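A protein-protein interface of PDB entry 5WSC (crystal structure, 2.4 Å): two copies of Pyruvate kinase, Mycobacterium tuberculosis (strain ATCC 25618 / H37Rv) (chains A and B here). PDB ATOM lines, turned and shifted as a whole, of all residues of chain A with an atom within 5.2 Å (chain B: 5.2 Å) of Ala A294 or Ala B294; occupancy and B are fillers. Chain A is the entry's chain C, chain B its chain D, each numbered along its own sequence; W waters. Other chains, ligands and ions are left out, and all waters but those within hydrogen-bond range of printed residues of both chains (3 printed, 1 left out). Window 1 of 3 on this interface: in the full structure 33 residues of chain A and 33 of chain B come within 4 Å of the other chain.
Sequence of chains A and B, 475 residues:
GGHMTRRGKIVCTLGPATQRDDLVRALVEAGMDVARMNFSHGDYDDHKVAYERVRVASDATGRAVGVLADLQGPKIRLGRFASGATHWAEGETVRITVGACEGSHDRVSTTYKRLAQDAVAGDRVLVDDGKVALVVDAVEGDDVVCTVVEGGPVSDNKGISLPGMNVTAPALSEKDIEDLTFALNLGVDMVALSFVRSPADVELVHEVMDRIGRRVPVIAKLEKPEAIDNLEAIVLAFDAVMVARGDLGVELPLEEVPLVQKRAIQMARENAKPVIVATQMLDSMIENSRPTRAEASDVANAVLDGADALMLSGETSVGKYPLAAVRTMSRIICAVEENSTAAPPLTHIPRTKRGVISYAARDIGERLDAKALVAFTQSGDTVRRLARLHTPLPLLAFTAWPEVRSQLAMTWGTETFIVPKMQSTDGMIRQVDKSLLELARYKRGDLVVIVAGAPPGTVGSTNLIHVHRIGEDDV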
ATOM      1  N   ARG A 245       8.364  -9.317 -34.442  1.00  0.00           N
ATOM      2  CA  ARG A 245       7.145 -10.031 -34.110  1.00  0.00           C
ATOM      3  C   ARG A 245       6.080  -9.959 -35.203  1.00  0.00           C
ATOM      4  O   ARG A 245       5.212 -10.816 -35.278  1.00  0.00           O
ATOM      5  CB  ARG A 245       6.579  -9.491 -32.805  1.00  0.00           C
ATOM      6  CG  ARG A 245       7.613  -9.447 -31.689  1.00  0.00           C
ATOM      7  CD  ARG A 245       7.049  -9.030 -30.346  1.00  0.00           C
ATOM      8  NE  ARG A 245       6.288  -7.801 -30.429  1.00  0.00           N
ATOM      9  CZ  ARG A 245       5.634  -7.284 -29.392  1.00  0.00           C
ATOM     10  NH1 ARG A 245       4.923  -6.180 -29.549  1.00  0.00           N
ATOM     11  NH2 ARG A 245       5.694  -7.872 -28.181  1.00  0.00           N
ATOM     12  N   GLN A 280       4.545  -3.435 -33.513  1.00  0.00           N
ATOM     13  CA  GLN A 280       3.227  -3.279 -32.927  1.00  0.00           C
ATOM     14  C   GLN A 280       3.171  -3.111 -31.399  1.00  0.00           C
ATOM     15  O   GLN A 280       2.120  -3.360 -30.796  1.00  0.00           O
ATOM     16  CB  GLN A 280       2.340  -4.456 -33.341  1.00  0.00           C
ATOM     17  CG  GLN A 280       2.059  -4.473 -34.845  1.00  0.00           C
ATOM     18  CD  GLN A 280       1.138  -5.573 -35.293  1.00  0.00           C
ATOM     19  OE1 GLN A 280       0.885  -6.547 -34.581  1.00  0.00           O
ATOM     20  NE2 GLN A 280       0.590  -5.399 -36.462  1.00  0.00           N
ATOM     21  N   MET A 281       4.285  -2.703 -30.776  1.00  0.00           N
ATOM     22  CA  MET A 281       4.302  -2.461 -29.350  1.00  0.00           C
ATOM     23  C   MET A 281       3.373  -1.327 -29.017  1.00  0.00           C
ATOM     24  O   MET A 281       2.743  -1.326 -27.959  1.00  0.00           O
ATOM     25  CB  MET A 281       5.718  -2.103 -28.847  1.00  0.00           C
ATOM     26  CG  MET A 281       6.805  -3.105 -29.231  1.00  0.00           C
ATOM     27  SD  MET A 281       8.155  -3.193 -27.988  1.00  0.00           S
ATOM     28  CE  MET A 281       7.278  -4.058 -26.706  1.00  0.00           C
ATOM     29  N   THR A 292      -3.528   1.590 -26.390  1.00  0.00           N
ATOM     30  CA  THR A 292      -4.406   0.708 -25.659  1.00  0.00           C
ATOM     31  C   THR A 292      -3.706   0.242 -24.375  1.00  0.00           C
ATOM     32  O   THR A 292      -2.487   0.484 -24.154  1.00  0.00           O
ATOM     33  CB  THR A 292      -4.801  -0.517 -26.503  1.00  0.00           C
ATOM     34  OG1 THR A 292      -3.686  -1.385 -26.647  1.00  0.00           O
ATOM     35  CG2 THR A 292      -5.239  -0.097 -27.886  1.00  0.00           C
ATOM     36  N   ARG A 293      -4.484  -0.409 -23.523  1.00  0.00           N
ATOM     37  CA  ARG A 293      -3.980  -0.962 -22.271  1.00  0.00           C
ATOM     38  C   ARG A 293      -3.073  -2.161 -22.534  1.00  0.00           C
ATOM     39  O   ARG A 293      -2.119  -2.374 -21.795  1.00  0.00           O
ATOM     40  CB  ARG A 293      -5.148  -1.399 -21.433  1.00  0.00           C
ATOM     41  CG  ARG A 293      -6.080  -0.273 -21.065  1.00  0.00           C
ATOM     42  CD  ARG A 293      -5.334   0.826 -20.331  1.00  0.00           C
ATOM     43  NE  ARG A 293      -6.229   1.945 -20.138  1.00  0.00           N
ATOM     44  CZ  ARG A 293      -6.292   3.010 -20.923  1.00  0.00           C
ATOM     45  NH1 ARG A 293      -5.421   3.179 -21.932  1.00  0.00           N
ATOM     46  NH2 ARG A 293      -7.202   3.944 -20.649  1.00  0.00           N
ATOM     47  N   ALA A 294      -3.382  -2.932 -23.585  1.00  0.00           N
ATOM     48  CA  ALA A 294      -2.532  -4.031 -24.041  1.00  0.00           C
ATOM     49  C   ALA A 294      -1.174  -3.579 -24.558  1.00  0.00           C
ATOM     50  O   ALA A 294      -0.172  -4.263 -24.413  1.00  0.00           O
ATOM     51  CB  ALA A 294      -3.262  -4.808 -25.141  1.00  0.00           C
ATOM     52  N   GLU A 295      -1.162  -2.465 -25.258  1.00  0.00           N
ATOM     53  CA  GLU A 295       0.093  -1.887 -25.732  1.00  0.00           C
ATOM     54  C   GLU A 295       0.965  -1.467 -24.564  1.00  0.00           C
ATOM     55  O   GLU A 295       2.115  -1.885 -24.463  1.00  0.00           O
ATOM     56  CB  GLU A 295      -0.185  -0.770 -26.702  1.00  0.00           C
ATOM     57  CG  GLU A 295      -0.586  -1.307 -28.059  1.00  0.00           C
ATOM     58  CD  GLU A 295      -1.350  -0.321 -28.933  1.00  0.00           C
ATOM     59  OE1 GLU A 295      -1.572   0.859 -28.522  1.00  0.00           O
ATOM     60  OE2 GLU A 295      -1.697  -0.749 -30.058  1.00  0.00           O
ATOM     61  N   ALA A 296       0.410  -0.689 -23.652  1.00  0.00           N
ATOM     62  CA  ALA A 296       1.161  -0.222 -22.469  1.00  0.00           C
ATOM     63  C   ALA A 296       1.728  -1.426 -21.717  1.00  0.00           C
ATOM     64  O   ALA A 296       2.913  -1.476 -21.373  1.00  0.00           O
ATOM     65  CB  ALA A 296       0.255   0.572 -21.573  1.00  0.00           C
ATOM     66  N   SER A 297       0.876  -2.409 -21.476  1.00  0.00           N
ATOM     67  CA  SER A 297       1.300  -3.666 -20.894  1.00  0.00           C
ATOM     68  C   SER A 297       2.459  -4.305 -21.665  1.00  0.00           C
ATOM     69  O   SER A 297       3.445  -4.799 -21.049  1.00  0.00           O
ATOM     70  CB  SER A 297       0.103  -4.628 -20.871  1.00  0.00           C
ATOM     71  OG  SER A 297       0.458  -5.898 -20.342  1.00  0.00           O
ATOM     72  N   ASP A 298       2.334  -4.342 -22.994  1.00  0.00           N
ATOM     73  CA  ASP A 298       3.273  -5.085 -23.826  1.00  0.00           C
ATOM     74  C   ASP A 298       4.669  -4.519 -23.642  1.00  0.00           C
ATOM     75  O   ASP A 298       5.656  -5.267 -23.446  1.00  0.00           O
ATOM     76  CB  ASP A 298       2.844  -5.003 -25.301  1.00  0.00           C
ATOM     77  CG  ASP A 298       3.771  -5.706 -26.212  1.00  0.00           C
ATOM     78  OD1 ASP A 298       4.170  -6.792 -25.883  1.00  0.00           O
ATOM     79  OD2 ASP A 298       4.095  -5.176 -27.296  1.00  0.00           O
ATOM     80  N   VAL A 299       4.728  -3.188 -23.664  1.00  0.00           N
ATOM     81  CA  VAL A 299       5.935  -2.432 -23.424  1.00  0.00           C
ATOM     82  C   VAL A 299       6.498  -2.656 -22.026  1.00  0.00           C
ATOM     83  O   VAL A 299       7.689  -2.846 -21.874  1.00  0.00           O
ATOM     84  CB  VAL A 299       5.665  -0.915 -23.665  1.00  0.00           C
ATOM     85  CG1 VAL A 299       6.762  -0.038 -23.089  1.00  0.00           C
ATOM     86  CG2 VAL A 299       5.520  -0.640 -25.169  1.00  0.00           C
ATOM     87  N   ARG B 245      -9.140  -1.783 -16.488  1.00  0.00           N
ATOM     88  CA  ARG B 245      -8.001  -1.002 -16.932  1.00  0.00           C
ATOM     89  C   ARG B 245      -8.393   0.184 -17.817  1.00  0.00           C
ATOM     90  O   ARG B 245      -7.651   1.163 -17.908  1.00  0.00           O
ATOM     91  CB  ARG B 245      -7.019  -1.911 -17.676  1.00  0.00           C
ATOM     92  CG  ARG B 245      -6.662  -3.155 -16.889  1.00  0.00           C
ATOM     93  CD  ARG B 245      -5.590  -4.005 -17.554  1.00  0.00           C
ATOM     94  NE  ARG B 245      -5.931  -4.328 -18.931  1.00  0.00           N
ATOM     95  CZ  ARG B 245      -5.142  -5.015 -19.737  1.00  0.00           C
ATOM     96  NH1 ARG B 245      -5.500  -5.205 -20.984  1.00  0.00           N
ATOM     97  NH2 ARG B 245      -3.970  -5.484 -19.307  1.00  0.00           N
ATOM     98  N   GLN B 280      -9.648  -4.016 -23.163  1.00  0.00           N
ATOM     99  CA  GLN B 280      -8.703  -3.824 -24.251  1.00  0.00           C
ATOM    100  C   GLN B 280      -7.584  -4.857 -24.382  1.00  0.00           C
ATOM    101  O   GLN B 280      -6.561  -4.574 -25.013  1.00  0.00           O
ATOM    102  CB  GLN B 280      -8.087  -2.437 -24.148  1.00  0.00           C
ATOM    103  CG  GLN B 280      -9.071  -1.293 -24.395  1.00  0.00           C
ATOM    104  CD  GLN B 280      -8.413   0.056 -24.210  1.00  0.00           C
ATOM    105  OE1 GLN B 280      -7.216   0.223 -24.542  1.00  0.00           O
ATOM    106  NE2 GLN B 280      -9.172   1.041 -23.685  1.00  0.00           N
ATOM    107  N   MET B 281      -7.776  -6.047 -23.819  1.00  0.00           N
ATOM    108  CA  MET B 281      -6.812  -7.124 -23.951  1.00  0.00           C
ATOM    109  C   MET B 281      -6.707  -7.518 -25.392  1.00  0.00           C
ATOM    110  O   MET B 281      -5.634  -7.915 -25.855  1.00  0.00           O
ATOM    111  CB  MET B 281      -7.247  -8.365 -23.119  1.00  0.00           C
ATOM    112  CG  MET B 281      -7.568  -8.054 -21.659  1.00  0.00           C
ATOM    113  SD  MET B 281      -7.125  -9.359 -20.460  1.00  0.00           S
ATOM    114  CE  MET B 281      -5.369  -9.369 -20.583  1.00  0.00           C
ATOM    115  N   THR B 292      -3.149  -7.681 -32.522  1.00  0.00           N
ATOM    116  CA  THR B 292      -1.783  -7.231 -32.610  1.00  0.00           C
ATOM    117  C   THR B 292      -0.888  -8.152 -31.753  1.00  0.00           C
ATOM    118  O   THR B 292      -1.366  -9.020 -30.991  1.00  0.00           O
ATOM    119  CB  THR B 292      -1.652  -5.780 -32.114  1.00  0.00           C
ATOM    120  OG1 THR B 292      -1.830  -5.740 -30.711  1.00  0.00           O
ATOM    121  CG2 THR B 292      -2.712  -4.895 -32.709  1.00  0.00           C
ATOM    122  N   ARG B 293       0.411  -7.951 -31.888  1.00  0.00           N
ATOM    123  CA  ARG B 293       1.404  -8.678 -31.108  1.00  0.00           C
ATOM    124  C   ARG B 293       1.390  -8.212 -29.652  1.00  0.00           C
ATOM    125  O   ARG B 293       1.650  -9.013 -28.759  1.00  0.00           O
ATOM    126  CB  ARG B 293       2.760  -8.421 -31.693  1.00  0.00           C
ATOM    127  CG  ARG B 293       2.919  -8.858 -33.127  1.00  0.00           C
ATOM    128  CD  ARG B 293       2.574 -10.316 -33.290  1.00  0.00           C
ATOM    129  NE  ARG B 293       2.613 -10.712 -34.672  1.00  0.00           N
ATOM    130  CZ  ARG B 293       1.579 -10.680 -35.518  1.00  0.00           C
ATOM    131  NH1 ARG B 293       0.370 -10.293 -35.125  1.00  0.00           N
ATOM    132  NH2 ARG B 293       1.765 -11.079 -36.781  1.00  0.00           N
ATOM    133  N   ALA B 294       1.097  -6.921 -29.420  1.00  0.00           N
ATOM    134  CA  ALA B 294       0.892  -6.388 -28.059  1.00  0.00           C
ATOM    135  C   ALA B 294      -0.305  -6.992 -27.328  1.00  0.00           C
ATOM    136  O   ALA B 294      -0.306  -7.176 -26.128  1.00  0.00           O
ATOM    137  CB  ALA B 294       0.720  -4.874 -28.113  1.00  0.00           C
ATOM    138  N   GLU B 295      -1.374  -7.210 -28.057  1.00  0.00           N
ATOM    139  CA  GLU B 295      -2.552  -7.830 -27.496  1.00  0.00           C
ATOM    140  C   GLU B 295      -2.258  -9.257 -27.095  1.00  0.00           C
ATOM    141  O   GLU B 295      -2.506  -9.640 -25.941  1.00  0.00           O
ATOM    142  CB  GLU B 295      -3.700  -7.712 -28.463  1.00  0.00           C
ATOM    143  CG  GLU B 295      -4.283  -6.310 -28.437  1.00  0.00           C
ATOM    144  CD  GLU B 295      -5.097  -5.943 -29.659  1.00  0.00           C
ATOM    145  OE1 GLU B 295      -5.267  -6.802 -30.597  1.00  0.00           O
ATOM    146  OE2 GLU B 295      -5.559  -4.774 -29.656  1.00  0.00           O
ATOM    147  N   ALA B 296      -1.682 -10.034 -28.008  1.00  0.00           N
ATOM    148  CA  ALA B 296      -1.322 -11.432 -27.708  1.00  0.00           C
ATOM    149  C   ALA B 296      -0.456 -11.485 -26.459  1.00  0.00           C
ATOM    150  O   ALA B 296      -0.710 -12.244 -25.524  1.00  0.00           O
ATOM    151  CB  ALA B 296      -0.595 -12.035 -28.880  1.00  0.00           C
ATOM    152  N   SER B 297       0.576 -10.658 -26.445  1.00  0.00           N
ATOM    153  CA  SER B 297       1.430 -10.507 -25.292  1.00  0.00           C
ATOM    154  C   SER B 297       0.640 -10.182 -24.031  1.00  0.00           C
ATOM    155  O   SER B 297       0.931 -10.735 -22.933  1.00  0.00           O
ATOM    156  CB  SER B 297       2.433  -9.372 -25.570  1.00  0.00           C
ATOM    157  OG  SER B 297       3.266  -9.115 -24.446  1.00  0.00           O
ATOM    158  N   ASP B 298      -0.306  -9.246 -24.141  1.00  0.00           N
ATOM    159  CA  ASP B 298      -0.963  -8.708 -22.962  1.00  0.00           C
ATOM    160  C   ASP B 298      -1.703  -9.835 -22.253  1.00  0.00           C
ATOM    161  O   ASP B 298      -1.613 -10.006 -21.013  1.00  0.00           O
ATOM    162  CB  ASP B 298      -1.942  -7.601 -23.361  1.00  0.00           C
ATOM    163  CG  ASP B 298      -2.693  -7.044 -22.178  1.00  0.00           C
ATOM    164  OD1 ASP B 298      -2.085  -6.828 -21.153  1.00  0.00           O
ATOM    165  OD2 ASP B 298      -3.900  -6.816 -22.266  1.00  0.00           O
ATOM    166  N   VAL B 299      -2.403 -10.625 -23.069  1.00  0.00           N
ATOM    167  CA  VAL B 299      -3.104 -11.797 -22.631  1.00  0.00           C
ATOM    168  C   VAL B 299      -2.169 -12.853 -22.036  1.00  0.00           C
ATOM    169  O   VAL B 299      -2.480 -13.421 -21.010  1.00  0.00           O
ATOM    170  CB  VAL B 299      -3.920 -12.393 -23.818  1.00  0.00           C
ATOM    171  CG1 VAL B 299      -4.386 -13.813 -23.540  1.00  0.00           C
ATOM    172  CG2 VAL B 299      -5.118 -11.502 -24.123  1.00  0.00           C
HETATM  173  O   HOH W   1       5.783  -7.779 -24.340  1.00  0.00           O
HETATM  174  O   HOH W   2      -5.437  -3.394 -27.543  1.00  0.00           O
HETATM  175  O   HOH W   3      -1.453  -8.070 -18.890  1.00  0.00           O
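The guanidinium group (NE) of Arg B293 sits at hydrogen-bond distance from the backbone carbonyl oxygen (O) of Arg A245 (2.7 Å).
The side-chain amide oxygen of Gln A280 is in hydrogen-bond range of the backbone NH of Arg B293, at 3.1 Å.
NE of Arg A293 sits at hydrogen-bond distance from O of Arg B245 (2.8 Å).
N of Arg A293 lies within hydrogen-bond range of OE1 of Gln B280 (3.0 Å).
OD1 of Asp B298 lies within hydrogen-bond range of OG of Ser A297.
The side-chain hydroxyl of Ser B297 lies within hydrogen-bond range of the side-chain carboxylate of Asp A298 (2.9 Å).
The backbone carbonyl oxygen (O) of Ala A294 lies close to the backbone carbonyl oxygen (O) of Ala B294.
The guanidinium group (NH1) of Arg A245 is in salt-bridge range of the side-chain carboxylate (OD2) of Asp A298, at 2.6 Å.
OG1 of Thr A292 lies close to N of Ala A294, 3.4 Å away.
The backbone NH (N) of Thr A292 is in hydrogen-bond range of the side-chain carboxylate (OE1) of Glu A295.
NH1 of Arg B245 is in salt-bridge range of OD2 of Asp B298, 2.6 Å away.
The backbone NH of Ala B294 lies close to the side-chain hydroxyl of Thr B292 (3.4 Å).
The backbone NH (N) of Thr B292 lies within hydrogen-bond range of the side-chain carboxylate (OE1) of Glu B295, at 3.0 Å.
Among the printed residues, pairs that only touch across the chains: Arg A245 with Ala B294, Gln A280 with Thr B292, Gln A280 with Ala B294, Thr A292 with Gln B280, Ala A294 with Gln B280, Ala A294 with Met B281, Ala A294 with Glu B295, Ala A294 with Asp B298, Glu A295 with Ala B294 and Asp A298 with Ala B294.
Of the printed residues of chain B, Asp A298 touches Ala B294 (3.5 Å) and Ser B297 (2.9 Å).
Val A299 touches none of the printed residues of chain B.
Printed residues of chain A within 4 Å of Thr B292: Gln A280 (3.4 Å).
Of chain A, only Arg A245, Gln A280, Ala A294, Glu A295 and Asp A298 come within 4 Å of Ala B294.
Of the printed residues of chain A, Glu B295 touches Ala A294.
Ala B296 touches none of the printed residues of chain A.
Printed residues of chain A within 4 Å of Ser B297: Asp A298 (2.9 Å).
The nearest printed residue of chain B that does not touch Ser A297 is Arg B245 (4.4 Å).
Of the 11 printed residues of chain B, 9 touch a printed residue of chain A.
Hydrophobic or aromatic side chains of chain B within 4 Å of the printed part of chain A: Ala B294.
Of the 11 printed residues of chain A, 8 touch a printed residue of chain B.
Along chain A the printed residues that touch a printed residue of chain B span positions 245 to 298.
Among the printed residues, 17 pairs touch across the chains.
Among the printed residues, no Asp or Glu carboxylate lies within 4 Å of a Lys or Arg side-chain nitrogen of the other chain.
Arg A245 touches Arg B293, and with the chains exchanged Arg A293 touches Arg B245.
Gln A280 touches Thr B292, and with the chains exchanged Thr A292 touches Gln B280.
Ala A294 touches Met B281, but with the chains exchanged Met A281 does not touch Ala B294 (4.1 Å).
Ala B294 touches its own counterpart, Ala A294.
Positions printed for both chains: 245, 280, 281, 292, 293, 294, 295, 296, 297, 298 and 299.
Water W1 bridges OD1 of Asp A298 and OG of Ser B297.
Water W2 lies within hydrogen-bond range of OE2 of Glu B295 (2.5 Å), OG1 of Thr A292 (2.8 Å) and O of Gln B280 (3.0 Å).
Water W3 bridges the side-chain carboxylate (OD1) of Asp B298 (2.7 Å) and the side-chain hydroxyl (OG) of Ser A297 (3.2 Å).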
